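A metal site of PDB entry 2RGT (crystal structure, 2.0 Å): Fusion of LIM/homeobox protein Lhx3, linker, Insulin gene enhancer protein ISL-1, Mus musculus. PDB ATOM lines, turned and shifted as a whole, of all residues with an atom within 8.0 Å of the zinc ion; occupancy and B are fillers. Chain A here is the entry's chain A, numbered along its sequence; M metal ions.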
ATOM      1  N   ALA A  95       3.096  -8.791 -20.439  1.00  0.00           N
ATOM      2  CA  ALA A  95       3.705  -9.539 -21.511  1.00  0.00           C
ATOM      3  C   ALA A  95       5.044 -10.054 -20.931  1.00  0.00           C
ATOM      4  O   ALA A  95       5.610  -9.466 -19.959  1.00  0.00           O
ATOM      5  CB  ALA A  95       3.925  -8.644 -22.781  1.00  0.00           C
ATOM      6  N   CYS A  96       5.494 -11.219 -21.436  1.00  0.00           N
ATOM      7  CA  CYS A  96       6.843 -11.694 -21.046  1.00  0.00           C
ATOM      8  C   CYS A  96       7.986 -10.737 -21.464  1.00  0.00           C
ATOM      9  O   CYS A  96       8.137 -10.362 -22.616  1.00  0.00           O
ATOM     10  CB  CYS A  96       7.090 -13.117 -21.555  1.00  0.00           C
ATOM     11  SG  CYS A  96       8.740 -13.906 -21.118  1.00  0.00           S
ATOM     12  N   VAL A  97       8.841 -10.382 -20.523  1.00  0.00           N
ATOM     13  CA  VAL A  97       9.935  -9.473 -20.787  1.00  0.00           C
ATOM     14  C   VAL A  97      11.054 -10.079 -21.677  1.00  0.00           C
ATOM     15  O   VAL A  97      11.812  -9.357 -22.366  1.00  0.00           O
ATOM     16  CB  VAL A  97      10.460  -8.862 -19.433  1.00  0.00           C
ATOM     17  CG1 VAL A  97      11.393  -9.856 -18.712  1.00  0.00           C
ATOM     18  CG2 VAL A  97      11.154  -7.547 -19.702  1.00  0.00           C
ATOM     19  N   VAL A  98      11.090 -11.406 -21.757  1.00  0.00           N
ATOM     20  CA  VAL A  98      12.049 -12.146 -22.619  1.00  0.00           C
ATOM     21  C   VAL A  98      11.525 -12.381 -24.048  1.00  0.00           C
ATOM     22  O   VAL A  98      12.160 -11.955 -25.033  1.00  0.00           O
ATOM     23  CB  VAL A  98      12.431 -13.497 -21.957  1.00  0.00           C
ATOM     24  CG1 VAL A  98      13.437 -14.259 -22.824  1.00  0.00           C
ATOM     25  CG2 VAL A  98      12.977 -13.216 -20.542  1.00  0.00           C
ATOM     26  N   CYS A  99      10.395 -13.064 -24.185  1.00  0.00           N
ATOM     27  CA  CYS A  99       9.861 -13.319 -25.533  1.00  0.00           C
ATOM     28  C   CYS A  99       8.859 -12.251 -26.025  1.00  0.00           C
ATOM     29  O   CYS A  99       8.485 -12.258 -27.205  1.00  0.00           O
ATOM     30  CB  CYS A  99       9.267 -14.719 -25.608  1.00  0.00           C
ATOM     31  SG  CYS A  99       7.750 -14.917 -24.673  1.00  0.00           S
ATOM     32  N   LYS A 100       8.392 -11.377 -25.142  1.00  0.00           N
ATOM     33  CA  LYS A 100       7.461 -10.238 -25.483  1.00  0.00           C
ATOM     34  C   LYS A 100       5.995 -10.689 -25.775  1.00  0.00           C
ATOM     35  O   LYS A 100       5.150  -9.892 -26.106  1.00  0.00           O
ATOM     36  CB  LYS A 100       8.001  -9.340 -26.620  1.00  0.00           C
ATOM     37  CG  LYS A 100       9.558  -9.085 -26.656  1.00  0.00           C
ATOM     38  CD  LYS A 100      10.016  -8.248 -25.423  1.00  0.00           C
ATOM     39  CE  LYS A 100      11.574  -8.031 -25.389  1.00  0.00           C
ATOM     40  NZ  LYS A 100      11.893  -7.338 -24.066  1.00  0.00           N
ATOM     41  N   ARG A 101       5.704 -11.978 -25.651  1.00  0.00           N
ATOM     42  CA  ARG A 101       4.354 -12.510 -25.765  1.00  0.00           C
ATOM     43  C   ARG A 101       3.437 -11.990 -24.645  1.00  0.00           C
ATOM     44  O   ARG A 101       3.837 -11.926 -23.449  1.00  0.00           O
ATOM     45  CB  ARG A 101       4.374 -14.039 -25.760  1.00  0.00           C
ATOM     46  CG  ARG A 101       3.032 -14.720 -26.016  1.00  0.00           C
ATOM     47  CD  ARG A 101       3.185 -16.224 -25.887  1.00  0.00           C
ATOM     48  NE  ARG A 101       3.559 -16.727 -24.533  1.00  0.00           N
ATOM     49  CZ  ARG A 101       2.698 -17.031 -23.546  1.00  0.00           C
ATOM     50  NH1 ARG A 101       1.394 -16.849 -23.691  1.00  0.00           N
ATOM     51  NH2 ARG A 101       3.153 -17.510 -22.388  1.00  0.00           N
ATOM     52  N   GLN A 102       2.231 -11.564 -25.087  1.00  0.00           N
ATOM     53  CA  GLN A 102       1.216 -10.980 -24.229  1.00  0.00           C
ATOM     54  C   GLN A 102       0.655 -12.124 -23.431  1.00  0.00           C
ATOM     55  O   GLN A 102       0.303 -13.129 -23.980  1.00  0.00           O
ATOM     56  CB  GLN A 102       0.119 -10.226 -25.048  1.00  0.00           C
ATOM     57  CG  GLN A 102      -0.422  -8.950 -24.316  1.00  0.00           C
ATOM     58  CD  GLN A 102      -1.642  -8.238 -25.005  1.00  0.00           C
ATOM     59  OE1 GLN A 102      -1.459  -7.351 -25.885  1.00  0.00           O
ATOM     60  NE2 GLN A 102      -2.871  -8.591 -24.599  1.00  0.00           N
ATOM     61  N   LEU A 103       0.616 -12.001 -22.111  1.00  0.00           N
ATOM     62  CA  LEU A 103       0.110 -13.106 -21.353  1.00  0.00           C
ATOM     63  C   LEU A 103      -1.420 -13.063 -21.251  1.00  0.00           C
ATOM     64  O   LEU A 103      -2.083 -12.014 -21.392  1.00  0.00           O
ATOM     65  CB  LEU A 103       0.746 -13.143 -19.972  1.00  0.00           C
ATOM     66  CG  LEU A 103       2.271 -13.117 -19.909  1.00  0.00           C
ATOM     67  CD1 LEU A 103       2.746 -12.869 -18.472  1.00  0.00           C
ATOM     68  CD2 LEU A 103       2.974 -14.326 -20.510  1.00  0.00           C
ATOM     69  N   GLU A 108       0.760 -19.508 -17.117  1.00  0.00           N
ATOM     70  CA  GLU A 108       1.762 -19.671 -16.082  1.00  0.00           C
ATOM     71  C   GLU A 108       2.949 -18.748 -16.349  1.00  0.00           C
ATOM     72  O   GLU A 108       3.532 -18.774 -17.443  1.00  0.00           O
ATOM     73  CB  GLU A 108       2.292 -21.124 -16.105  1.00  0.00           C
ATOM     74  CG  GLU A 108       1.359 -22.156 -15.476  1.00  0.00           C
ATOM     75  CD  GLU A 108       1.855 -23.538 -15.714  1.00  0.00           C
ATOM     76  OE1 GLU A 108       1.886 -23.964 -16.864  1.00  0.00           O
ATOM     77  OE2 GLU A 108       2.290 -24.208 -14.763  1.00  0.00           O
ATOM     78  N   LEU A 117       7.993  -9.614 -15.679  1.00  0.00           N
ATOM     79  CA  LEU A 117       7.153 -10.744 -15.883  1.00  0.00           C
ATOM     80  C   LEU A 117       7.863 -11.635 -16.855  1.00  0.00           C
ATOM     81  O   LEU A 117       8.317 -11.177 -17.902  1.00  0.00           O
ATOM     82  CB  LEU A 117       5.828 -10.313 -16.501  1.00  0.00           C
ATOM     83  CG  LEU A 117       4.927  -9.376 -15.695  1.00  0.00           C
ATOM     84  CD1 LEU A 117       3.696  -8.846 -16.482  1.00  0.00           C
ATOM     85  CD2 LEU A 117       4.463 -10.088 -14.469  1.00  0.00           C
ATOM     86  N   VAL A 118       7.925 -12.930 -16.529  1.00  0.00           N
ATOM     87  CA  VAL A 118       8.637 -13.936 -17.326  1.00  0.00           C
ATOM     88  C   VAL A 118       7.704 -15.142 -17.439  1.00  0.00           C
ATOM     89  O   VAL A 118       7.291 -15.691 -16.406  1.00  0.00           O
ATOM     90  CB  VAL A 118       9.955 -14.411 -16.657  1.00  0.00           C
ATOM     91  CG1 VAL A 118      10.557 -15.450 -17.506  1.00  0.00           C
ATOM     92  CG2 VAL A 118      10.957 -13.285 -16.494  1.00  0.00           C
ATOM     93  N   CYS A 119       7.358 -15.545 -18.657  1.00  0.00           N
ATOM     94  CA  CYS A 119       6.547 -16.739 -18.843  1.00  0.00           C
ATOM     95  C   CYS A 119       7.323 -18.030 -18.356  1.00  0.00           C
ATOM     96  O   CYS A 119       8.565 -18.019 -18.197  1.00  0.00           O
ATOM     97  CB  CYS A 119       6.092 -16.894 -20.284  1.00  0.00           C
ATOM     98  SG  CYS A 119       7.366 -17.428 -21.457  1.00  0.00           S
ATOM     99  N   LYS A 120       6.575 -19.081 -18.087  1.00  0.00           N
ATOM    100  CA  LYS A 120       7.154 -20.287 -17.485  1.00  0.00           C
ATOM    101  C   LYS A 120       8.299 -20.804 -18.358  1.00  0.00           C
ATOM    102  O   LYS A 120       9.383 -21.069 -17.850  1.00  0.00           O
ATOM    103  CB  LYS A 120       6.051 -21.317 -17.224  1.00  0.00           C
ATOM    104  CG  LYS A 120       6.345 -22.385 -16.159  1.00  0.00           C
ATOM    105  CD  LYS A 120       6.732 -23.754 -16.764  1.00  0.00           C
ATOM    106  CE  LYS A 120       5.724 -24.236 -17.846  1.00  0.00           C
ATOM    107  NZ  LYS A 120       5.946 -25.694 -18.239  1.00  0.00           N
ATOM    108  N   ALA A 121       8.080 -20.889 -19.681  1.00  0.00           N
ATOM    109  CA  ALA A 121       9.036 -21.422 -20.655  1.00  0.00           C
ATOM    110  C   ALA A 121      10.352 -20.669 -20.687  1.00  0.00           C
ATOM    111  O   ALA A 121      11.340 -21.221 -21.105  1.00  0.00           O
ATOM    112  CB  ALA A 121       8.421 -21.448 -22.071  1.00  0.00           C
ATOM    113  N   ASP A 122      10.360 -19.418 -20.235  1.00  0.00           N
ATOM    114  CA  ASP A 122      11.586 -18.610 -20.230  1.00  0.00           C
ATOM    115  C   ASP A 122      12.143 -18.423 -18.849  1.00  0.00           C
ATOM    116  O   ASP A 122      13.150 -17.769 -18.654  1.00  0.00           O
ATOM    117  CB  ASP A 122      11.297 -17.211 -20.837  1.00  0.00           C
ATOM    118  CG  ASP A 122      11.251 -17.226 -22.335  1.00  0.00           C
ATOM    119  OD1 ASP A 122      12.031 -17.917 -23.000  1.00  0.00           O
ATOM    120  OD2 ASP A 122      10.457 -16.465 -22.888  1.00  0.00           O
ATOM    121  N   TYR A 123      11.498 -18.994 -17.847  1.00  0.00           N
ATOM    122  CA  TYR A 123      11.941 -18.792 -16.484  1.00  0.00           C
ATOM    123  C   TYR A 123      13.346 -19.343 -16.144  1.00  0.00           C
ATOM    124  O   TYR A 123      14.114 -18.640 -15.491  1.00  0.00           O
ATOM    125  CB  TYR A 123      10.860 -19.224 -15.455  1.00  0.00           C
ATOM    126  CG  TYR A 123      11.378 -19.139 -14.022  1.00  0.00           C
ATOM    127  CD1 TYR A 123      11.546 -17.904 -13.399  1.00  0.00           C
ATOM    128  CD2 TYR A 123      11.763 -20.283 -13.335  1.00  0.00           C
ATOM    129  CE1 TYR A 123      12.023 -17.816 -12.109  1.00  0.00           C
ATOM    130  CE2 TYR A 123      12.262 -20.198 -12.043  1.00  0.00           C
ATOM    131  CZ  TYR A 123      12.388 -18.955 -11.449  1.00  0.00           C
ATOM    132  OH  TYR A 123      12.883 -18.825 -10.181  1.00  0.00           O
HETATM  133 ZN    ZN M   1       8.405 -15.624 -22.615  1.00  0.00          ZN
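The side-chain sulfur (SG) of Cys 99 lies close to the backbone NH (N) of Arg 101. SG of Cys 96 sits close to N of Val 98 (3.5 Å). The backbone NH of Cys 96 lies within hydrogen-bond range of the backbone carbonyl oxygen of Arg 101.
Four residues have an atom within 4 Å of the zinc ion: Cys 96, Cys 99, Cys 119 and Asp 122.
OD2 of Asp 122 is bound to the zinc ion, at 2.2 Å. SG of Cys 99 is bound to the zinc ion. SG of Cys 96 binds the zinc ion (2.3 Å). SG of Cys 119 binds the zinc ion. The zinc ion has four donor atoms within binding distance.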
